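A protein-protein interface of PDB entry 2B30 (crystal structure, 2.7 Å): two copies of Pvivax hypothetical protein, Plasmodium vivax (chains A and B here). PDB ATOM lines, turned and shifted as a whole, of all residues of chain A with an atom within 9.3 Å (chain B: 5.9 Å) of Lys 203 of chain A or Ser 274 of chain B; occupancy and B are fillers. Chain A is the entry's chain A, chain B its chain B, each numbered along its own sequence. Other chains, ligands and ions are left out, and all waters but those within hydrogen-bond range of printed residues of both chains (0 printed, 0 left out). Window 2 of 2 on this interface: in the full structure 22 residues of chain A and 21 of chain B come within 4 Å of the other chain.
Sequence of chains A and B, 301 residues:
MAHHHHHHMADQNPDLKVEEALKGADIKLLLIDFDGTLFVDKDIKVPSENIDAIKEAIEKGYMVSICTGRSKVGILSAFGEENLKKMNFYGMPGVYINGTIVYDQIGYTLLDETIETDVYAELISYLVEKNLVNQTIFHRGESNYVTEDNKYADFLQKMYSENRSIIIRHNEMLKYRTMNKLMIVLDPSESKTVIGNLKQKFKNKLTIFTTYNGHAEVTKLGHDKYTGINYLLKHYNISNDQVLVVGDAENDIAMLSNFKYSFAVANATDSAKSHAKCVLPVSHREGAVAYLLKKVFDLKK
NZ of Lys 203 of chain A is in hydrogen-bond range of O of Ala 276 of chain B, at 2.5 Å. The backbone carbonyl oxygen of His 275 of chain B sits at hydrogen-bond distance from the side-chain amide nitrogen of Asn 204 of chain A, 3.1 Å away. The side-chain amide oxygen (OD1) of Asn 204 of chain A lies within hydrogen-bond range of the backbone NH (N) of Lys 277 of chain B (3.2 Å). NZ of Lys 203 of chain A sits close to O of Ser 274 of chain B (2.3 Å).
O of Asp 270 of chain B lies within hydrogen-bond range of OG of Ser 274 of chain B, at 2.9 Å. The side-chain hydroxyl of Ser 274 of chain B lies within hydrogen-bond range of the backbone carbonyl oxygen of Ser 271 of chain B (2.9 Å).
NZ of Lys 203 of chain A touches C of His 275 of chain B, at 3.9 Å. Ala 276 of chain B touches Asn 204 of chain A (C to OD1, 3.4 Å).
Lys 203 of chain A touches just these residues of chain B: Ser 274 (2.3 Å), His 275 (3.9 Å) and Ala 276 (2.5 Å). Ser 274 of chain B touches just one residue of chain A: Lys 203 (2.3 Å). No residue of chain A comes within 4 Å of Ser 271 of chain B. Printed residues of chain A within 4 Å of Ala 276 of chain B: Lys 203 and Asn 204. Printed residues of chain A within 4 Å of Lys 277 of chain B: Asn 204 (3.2 Å). Of the printed residues of chain A, His 275 of chain B touches Lys 203 (3.9 Å) and Asn 204 (3.1 Å). Of the printed residues of chain B, Asn 204 of chain A touches His 275 (3.1 Å), Ala 276 (3.4 Å) and Lys 277 (3.2 Å). Lys 199 of chain A touches none of the printed residues of chain B. Ile 195 of chain A touches none of the printed residues of chain B. The nearest printed residue of chain B that does not touch Lys 203 of chain A is Lys 277 of chain B (4.4 Å). The nearest printed residue of chain B that does not touch Asn 204 of chain A is Ser 274 of chain B (5.1 Å).
Of the 11 printed residues of chain B, 4 touch a printed residue of chain A. Of the 18 printed residues of chain A, 2 touch a printed residue of chain B. Among the printed residues, no Asp or Glu carboxylate lies within 4 Å of a Lys or Arg side-chain nitrogen of the other chain.
No position is printed for both chains. Of the 6 pairs that touch across the chains among the printed residues, none has its exchanged pair printed and touching as well.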
ATOM      1  N   VAL A 119       6.668 -31.769   2.779  1.00  0.00           N
ATOM      2  CA  VAL A 119       7.547 -30.688   3.260  1.00  0.00           C
ATOM      3  C   VAL A 119       8.931 -30.790   2.622  1.00  0.00           C
ATOM      4  O   VAL A 119       9.525 -29.774   2.282  1.00  0.00           O
ATOM      5  CB  VAL A 119       7.705 -30.688   4.813  1.00  0.00           C
ATOM      6  CG1 VAL A 119       8.579 -29.517   5.265  1.00  0.00           C
ATOM      7  CG2 VAL A 119       6.349 -30.616   5.497  1.00  0.00           C
ATOM      8  N   GLU A 122       8.905 -29.454  -0.833  1.00  0.00           N
ATOM      9  CA  GLU A 122       8.866 -28.014  -0.815  1.00  0.00           C
ATOM     10  C   GLU A 122      10.247 -27.502  -0.489  1.00  0.00           C
ATOM     11  O   GLU A 122      10.718 -26.543  -1.095  1.00  0.00           O
ATOM     12  CB  GLU A 122       7.848 -27.490   0.188  1.00  0.00           C
ATOM     13  CG  GLU A 122       7.659 -25.988   0.079  1.00  0.00           C
ATOM     14  CD  GLU A 122       6.454 -25.476   0.854  1.00  0.00           C
ATOM     15  OE1 GLU A 122       6.009 -26.160   1.809  1.00  0.00           O
ATOM     16  OE2 GLU A 122       5.952 -24.382   0.504  1.00  0.00           O
ATOM     17  N   LEU A 123      10.904 -28.167   0.452  1.00  0.00           N
ATOM     18  CA  LEU A 123      12.198 -27.716   0.940  1.00  0.00           C
ATOM     19  C   LEU A 123      13.233 -27.681  -0.176  1.00  0.00           C
ATOM     20  O   LEU A 123      13.949 -26.689  -0.329  1.00  0.00           O
ATOM     21  CB  LEU A 123      12.681 -28.612   2.081  1.00  0.00           C
ATOM     22  CG  LEU A 123      14.042 -28.273   2.670  1.00  0.00           C
ATOM     23  CD1 LEU A 123      14.004 -26.895   3.272  1.00  0.00           C
ATOM     24  CD2 LEU A 123      14.443 -29.317   3.699  1.00  0.00           C
ATOM     25  N   ILE A 195      19.244 -17.945   6.801  1.00  0.00           N
ATOM     26  CA  ILE A 195      18.495 -18.691   7.813  1.00  0.00           C
ATOM     27  C   ILE A 195      17.204 -17.965   8.166  1.00  0.00           C
ATOM     28  O   ILE A 195      16.155 -18.601   8.313  1.00  0.00           O
ATOM     29  CB  ILE A 195      19.312 -18.955   9.065  1.00  0.00           C
ATOM     30  CG1 ILE A 195      20.477 -19.888   8.722  1.00  0.00           C
ATOM     31  CG2 ILE A 195      18.429 -19.575  10.150  1.00  0.00           C
ATOM     32  CD1 ILE A 195      21.559 -19.926   9.776  1.00  0.00           C
ATOM     33  N   GLY A 196      17.273 -16.638   8.272  1.00  0.00           N
ATOM     34  CA  GLY A 196      16.074 -15.815   8.447  1.00  0.00           C
ATOM     35  C   GLY A 196      14.965 -16.186   7.480  1.00  0.00           C
ATOM     36  O   GLY A 196      13.879 -16.569   7.898  1.00  0.00           O
ATOM     37  N   ASN A 197      15.250 -16.096   6.184  1.00  0.00           N
ATOM     38  CA  ASN A 197      14.260 -16.432   5.141  1.00  0.00           C
ATOM     39  C   ASN A 197      13.847 -17.896   5.176  1.00  0.00           C
ATOM     40  O   ASN A 197      12.722 -18.243   4.802  1.00  0.00           O
ATOM     41  CB  ASN A 197      14.796 -16.105   3.743  1.00  0.00           C
ATOM     42  CG  ASN A 197      15.388 -14.714   3.657  1.00  0.00           C
ATOM     43  OD1 ASN A 197      14.791 -13.743   4.114  1.00  0.00           O
ATOM     44  ND2 ASN A 197      16.580 -14.614   3.088  1.00  0.00           N
ATOM     45  N   LEU A 198      14.772 -18.754   5.605  1.00  0.00           N
ATOM     46  CA  LEU A 198      14.491 -20.181   5.755  1.00  0.00           C
ATOM     47  C   LEU A 198      13.523 -20.415   6.926  1.00  0.00           C
ATOM     48  O   LEU A 198      12.537 -21.151   6.799  1.00  0.00           O
ATOM     49  CB  LEU A 198      15.799 -20.960   5.955  1.00  0.00           C
ATOM     50  CG  LEU A 198      15.800 -22.483   5.812  1.00  0.00           C
ATOM     51  CD1 LEU A 198      15.312 -22.931   4.440  1.00  0.00           C
ATOM     52  CD2 LEU A 198      17.207 -23.008   6.071  1.00  0.00           C
ATOM     53  N   LYS A 199      13.792 -19.758   8.051  1.00  0.00           N
ATOM     54  CA  LYS A 199      12.945 -19.891   9.237  1.00  0.00           C
ATOM     55  C   LYS A 199      11.517 -19.358   9.071  1.00  0.00           C
ATOM     56  O   LYS A 199      10.658 -19.695   9.876  1.00  0.00           O
ATOM     57  CB  LYS A 199      13.602 -19.235  10.465  1.00  0.00           C
ATOM     58  CG  LYS A 199      14.756 -20.028  11.060  1.00  0.00           C
ATOM     59  CD  LYS A 199      15.049 -19.562  12.472  1.00  0.00           C
ATOM     60  CE  LYS A 199      16.225 -20.300  13.087  1.00  0.00           C
ATOM     61  NZ  LYS A 199      16.534 -19.790  14.451  1.00  0.00           N
ATOM     62  N   GLN A 200      11.256 -18.538   8.056  1.00  0.00           N
ATOM     63  CA  GLN A 200       9.896 -18.023   7.834  1.00  0.00           C
ATOM     64  C   GLN A 200       9.184 -18.727   6.680  1.00  0.00           C
ATOM     65  O   GLN A 200       7.956 -18.797   6.656  1.00  0.00           O
ATOM     66  CB  GLN A 200       9.887 -16.499   7.624  1.00  0.00           C
ATOM     67  CG  GLN A 200      10.773 -16.007   6.510  1.00  0.00           C
ATOM     68  CD  GLN A 200      10.607 -14.526   6.205  1.00  0.00           C
ATOM     69  OE1 GLN A 200      11.377 -13.963   5.416  1.00  0.00           O
ATOM     70  NE2 GLN A 200       9.610 -13.888   6.821  1.00  0.00           N
ATOM     71  N   LYS A 201       9.942 -19.229   5.714  1.00  0.00           N
ATOM     72  CA  LYS A 201       9.357 -20.068   4.674  1.00  0.00           C
ATOM     73  C   LYS A 201       8.865 -21.387   5.288  1.00  0.00           C
ATOM     74  O   LYS A 201       7.801 -21.891   4.910  1.00  0.00           O
ATOM     75  CB  LYS A 201      10.365 -20.343   3.556  1.00  0.00           C
ATOM     76  N   PHE A 202       9.634 -21.917   6.248  1.00  0.00           N
ATOM     77  CA  PHE A 202       9.336 -23.203   6.884  1.00  0.00           C
ATOM     78  C   PHE A 202       9.187 -23.074   8.409  1.00  0.00           C
ATOM     79  O   PHE A 202       9.575 -23.960   9.177  1.00  0.00           O
ATOM     80  CB  PHE A 202      10.413 -24.240   6.518  1.00  0.00           C
ATOM     81  CG  PHE A 202      10.576 -24.444   5.035  1.00  0.00           C
ATOM     82  CD1 PHE A 202       9.768 -25.348   4.348  1.00  0.00           C
ATOM     83  CD2 PHE A 202      11.527 -23.720   4.323  1.00  0.00           C
ATOM     84  CE1 PHE A 202       9.910 -25.523   2.975  1.00  0.00           C
ATOM     85  CE2 PHE A 202      11.676 -23.889   2.961  1.00  0.00           C
ATOM     86  CZ  PHE A 202      10.869 -24.795   2.283  1.00  0.00           C
ATOM     87  N   LYS A 203       8.605 -21.965   8.840  1.00  0.00           N
ATOM     88  CA  LYS A 203       8.175 -21.838  10.224  1.00  0.00           C
ATOM     89  C   LYS A 203       7.064 -22.865  10.485  1.00  0.00           C
ATOM     90  O   LYS A 203       6.229 -23.099   9.617  1.00  0.00           O
ATOM     91  CB  LYS A 203       7.653 -20.432  10.476  1.00  0.00           C
ATOM     92  CG  LYS A 203       7.751 -20.001  11.925  1.00  0.00           C
ATOM     93  CD  LYS A 203       6.671 -18.976  12.236  1.00  0.00           C
ATOM     94  CE  LYS A 203       6.357 -18.964  13.695  1.00  0.00           C
ATOM     95  NZ  LYS A 203       5.033 -18.356  13.902  1.00  0.00           N
ATOM     96  N   ASN A 204       7.074 -23.482  11.664  1.00  0.00           N
ATOM     97  CA  ASN A 204       6.142 -24.579  12.000  1.00  0.00           C
ATOM     98  C   ASN A 204       6.020 -25.667  10.914  1.00  0.00           C
ATOM     99  O   ASN A 204       4.957 -26.240  10.738  1.00  0.00           O
ATOM    100  CB  ASN A 204       4.729 -24.055  12.324  1.00  0.00           C
ATOM    101  CG  ASN A 204       4.690 -23.159  13.541  1.00  0.00           C
ATOM    102  OD1 ASN A 204       4.874 -21.948  13.434  1.00  0.00           O
ATOM    103  ND2 ASN A 204       4.412 -23.741  14.700  1.00  0.00           N
ATOM    104  N   LYS A 205       7.098 -25.927  10.181  1.00  0.00           N
ATOM    105  CA  LYS A 205       7.149 -27.018   9.207  1.00  0.00           C
ATOM    106  C   LYS A 205       8.444 -27.849   9.308  1.00  0.00           C
ATOM    107  O   LYS A 205       8.496 -28.994   8.845  1.00  0.00           O
ATOM    108  CB  LYS A 205       6.975 -26.448   7.799  1.00  0.00           C
ATOM    109  CG  LYS A 205       5.585 -25.853   7.579  1.00  0.00           C
ATOM    110  CD  LYS A 205       5.487 -25.009   6.324  1.00  0.00           C
ATOM    111  CE  LYS A 205       5.424 -25.857   5.067  1.00  0.00           C
ATOM    112  NZ  LYS A 205       5.070 -25.016   3.894  1.00  0.00           N
ATOM    113  N   LEU A 206       9.475 -27.272   9.925  1.00  0.00           N
ATOM    114  CA  LEU A 206      10.778 -27.914  10.088  1.00  0.00           C
ATOM    115  C   LEU A 206      11.456 -27.364  11.333  1.00  0.00           C
ATOM    116  O   LEU A 206      11.226 -26.222  11.727  1.00  0.00           O
ATOM    117  CB  LEU A 206      11.694 -27.622   8.888  1.00  0.00           C
ATOM    118  CG  LEU A 206      11.407 -28.312   7.550  1.00  0.00           C
ATOM    119  CD1 LEU A 206      12.165 -27.626   6.414  1.00  0.00           C
ATOM    120  CD2 LEU A 206      11.754 -29.794   7.621  1.00  0.00           C
ATOM    121  N   THR A 207      12.291 -28.195  11.940  1.00  0.00           N
ATOM    122  CA  THR A 207      13.221 -27.769  12.968  1.00  0.00           C
ATOM    123  C   THR A 207      14.481 -27.223  12.286  1.00  0.00           C
ATOM    124  O   THR A 207      15.153 -27.946  11.542  1.00  0.00           O
ATOM    125  CB  THR A 207      13.592 -28.977  13.832  1.00  0.00           C
ATOM    126  OG1 THR A 207      12.404 -29.493  14.435  1.00  0.00           O
ATOM    127  CG2 THR A 207      14.615 -28.622  14.898  1.00  0.00           C
ATOM    128  N   ILE A 208      14.797 -25.954  12.517  1.00  0.00           N
ATOM    129  CA  ILE A 208      16.002 -25.363  11.949  1.00  0.00           C
ATOM    130  C   ILE A 208      16.887 -24.812  13.058  1.00  0.00           C
ATOM    131  O   ILE A 208      16.600 -23.759  13.622  1.00  0.00           O
ATOM    132  CB  ILE A 208      15.689 -24.225  10.945  1.00  0.00           C
ATOM    133  CG1 ILE A 208      14.822 -24.724   9.784  1.00  0.00           C
ATOM    134  CG2 ILE A 208      16.980 -23.623  10.394  1.00  0.00           C
ATOM    135  CD1 ILE A 208      13.445 -24.070   9.716  1.00  0.00           C
ATOM    136  N   LEU A 221      10.098 -31.514  12.106  1.00  0.00           N
ATOM    137  CA  LEU A 221       9.479 -30.673  13.134  1.00  0.00           C
ATOM    138  C   LEU A 221       9.110 -31.493  14.352  1.00  0.00           C
ATOM    139  O   LEU A 221       8.725 -32.649  14.229  1.00  0.00           O
ATOM    140  CB  LEU A 221       8.212 -30.011  12.586  1.00  0.00           C
ATOM    141  CG  LEU A 221       7.495 -29.007  13.502  1.00  0.00           C
ATOM    142  CD1 LEU A 221       8.302 -27.739  13.654  1.00  0.00           C
ATOM    143  CD2 LEU A 221       6.107 -28.681  12.981  1.00  0.00           C
ATOM    144  N   THR B 269      -1.271 -14.397  23.946  1.00  0.00           N
ATOM    145  CA  THR B 269      -0.070 -13.635  24.257  1.00  0.00           C
ATOM    146  C   THR B 269       0.760 -13.419  23.006  1.00  0.00           C
ATOM    147  O   THR B 269       0.592 -14.125  22.018  1.00  0.00           O
ATOM    148  CB  THR B 269       0.822 -14.366  25.264  1.00  0.00           C
ATOM    149  OG1 THR B 269       0.023 -14.845  26.343  1.00  0.00           O
ATOM    150  CG2 THR B 269       1.906 -13.415  25.826  1.00  0.00           C
ATOM    151  N   ASP B 270       1.657 -12.442  23.055  1.00  0.00           N
ATOM    152  CA  ASP B 270       2.592 -12.187  21.955  1.00  0.00           C
ATOM    153  C   ASP B 270       3.433 -13.417  21.596  1.00  0.00           C
ATOM    154  O   ASP B 270       3.562 -13.765  20.421  1.00  0.00           O
ATOM    155  CB  ASP B 270       3.479 -10.979  22.282  1.00  0.00           C
ATOM    156  CG  ASP B 270       2.681  -9.686  22.368  1.00  0.00           C
ATOM    157  OD1 ASP B 270       1.768  -9.494  21.541  1.00  0.00           O
ATOM    158  OD2 ASP B 270       2.948  -8.857  23.257  1.00  0.00           O
ATOM    159  N   SER B 271       3.969 -14.090  22.604  1.00  0.00           N
ATOM    160  CA  SER B 271       4.787 -15.284  22.371  1.00  0.00           C
ATOM    161  C   SER B 271       3.974 -16.406  21.722  1.00  0.00           C
ATOM    162  O   SER B 271       4.393 -16.989  20.724  1.00  0.00           O
ATOM    163  CB  SER B 271       5.424 -15.779  23.677  1.00  0.00           C
ATOM    164  OG  SER B 271       6.169 -16.965  23.454  1.00  0.00           O
ATOM    165  N   ALA B 272       2.811 -16.700  22.290  1.00  0.00           N
ATOM    166  CA  ALA B 272       1.930 -17.710  21.735  1.00  0.00           C
ATOM    167  C   ALA B 272       1.695 -17.432  20.271  1.00  0.00           C
ATOM    168  O   ALA B 272       1.802 -18.335  19.445  1.00  0.00           O
ATOM    169  CB  ALA B 272       0.613 -17.730  22.477  1.00  0.00           C
ATOM    170  N   LYS B 273       1.385 -16.178  19.953  1.00  0.00           N
ATOM    171  CA  LYS B 273       1.105 -15.762  18.566  1.00  0.00           C
ATOM    172  C   LYS B 273       2.314 -15.945  17.642  1.00  0.00           C
ATOM    173  O   LYS B 273       2.156 -16.330  16.482  1.00  0.00           O
ATOM    174  CB  LYS B 273       0.618 -14.301  18.515  1.00  0.00           C
ATOM    175  CG  LYS B 273      -0.896 -14.131  18.624  1.00  0.00           C
ATOM    176  CD  LYS B 273      -1.320 -13.004  19.581  1.00  0.00           C
ATOM    177  CE  LYS B 273      -2.033 -11.852  18.903  1.00  0.00           C
ATOM    178  NZ  LYS B 273      -2.082 -10.650  19.808  1.00  0.00           N
ATOM    179  N   SER B 274       3.519 -15.682  18.140  1.00  0.00           N
ATOM    180  CA  SER B 274       4.700 -15.802  17.287  1.00  0.00           C
ATOM    181  C   SER B 274       5.110 -17.257  17.099  1.00  0.00           C
ATOM    182  O   SER B 274       5.582 -17.627  16.036  1.00  0.00           O
ATOM    183  CB  SER B 274       5.865 -14.953  17.801  1.00  0.00           C
ATOM    184  OG  SER B 274       5.947 -14.996  19.206  1.00  0.00           O
ATOM    185  N   HIS B 275       4.906 -18.089  18.111  1.00  0.00           N
ATOM    186  CA  HIS B 275       5.264 -19.507  18.008  1.00  0.00           C
ATOM    187  C   HIS B 275       4.259 -20.348  17.204  1.00  0.00           C
ATOM    188  O   HIS B 275       4.618 -21.421  16.687  1.00  0.00           O
ATOM    189  CB  HIS B 275       5.477 -20.083  19.404  1.00  0.00           C
ATOM    190  CG  HIS B 275       6.746 -19.614  20.049  1.00  0.00           C
ATOM    191  ND1 HIS B 275       7.936 -20.298  19.929  1.00  0.00           N
ATOM    192  CD2 HIS B 275       7.018 -18.514  20.789  1.00  0.00           C
ATOM    193  CE1 HIS B 275       8.883 -19.650  20.582  1.00  0.00           C
ATOM    194  NE2 HIS B 275       8.353 -18.563  21.111  1.00  0.00           N
ATOM    195  N   ALA B 276       3.018 -19.869  17.083  1.00  0.00           N
ATOM    196  CA  ALA B 276       2.003 -20.555  16.282  1.00  0.00           C
ATOM    197  C   ALA B 276       2.232 -20.330  14.798  1.00  0.00           C
ATOM    198  O   ALA B 276       2.774 -19.313  14.400  1.00  0.00           O
ATOM    199  CB  ALA B 276       0.604 -20.080  16.665  1.00  0.00           C
ATOM    200  N   LYS B 277       1.790 -21.271  13.976  1.00  0.00           N
ATOM    201  CA  LYS B 277       1.813 -21.087  12.532  1.00  0.00           C
ATOM    202  C   LYS B 277       0.980 -19.870  12.173  1.00  0.00           C
ATOM    203  O   LYS B 277       1.404 -19.013  11.401  1.00  0.00           O
ATOM    204  CB  LYS B 277       1.256 -22.317  11.805  1.00  0.00           C
ATOM    205  CG  LYS B 277       1.420 -22.277  10.279  1.00  0.00           C
ATOM    206  N   CYS B 278      -0.195 -19.787  12.780  1.00  0.00           N
ATOM    207  CA  CYS B 278      -1.196 -18.834  12.355  1.00  0.00           C
ATOM    208  C   CYS B 278      -2.025 -18.285  13.512  1.00  0.00           C
ATOM    209  O   CYS B 278      -2.504 -19.032  14.357  1.00  0.00           O
ATOM    210  CB  CYS B 278      -2.115 -19.523  11.357  1.00  0.00           C
ATOM    211  SG  CYS B 278      -3.406 -18.484  10.721  1.00  0.00           S
ATOM    212  N   VAL B 279      -2.198 -16.968  13.520  1.00  0.00           N
ATOM    213  CA  VAL B 279      -2.990 -16.280  14.528  1.00  0.00           C
ATOM    214  C   VAL B 279      -4.414 -16.146  14.013  1.00  0.00           C
ATOM    215  O   VAL B 279      -4.635 -15.625  12.925  1.00  0.00           O
ATOM    216  CB  VAL B 279      -2.436 -14.864  14.800  1.00  0.00           C
ATOM    217  CG1 VAL B 279      -3.217 -14.182  15.938  1.00  0.00           C
ATOM    218  CG2 VAL B 279      -0.941 -14.924  15.109  1.00  0.00           C
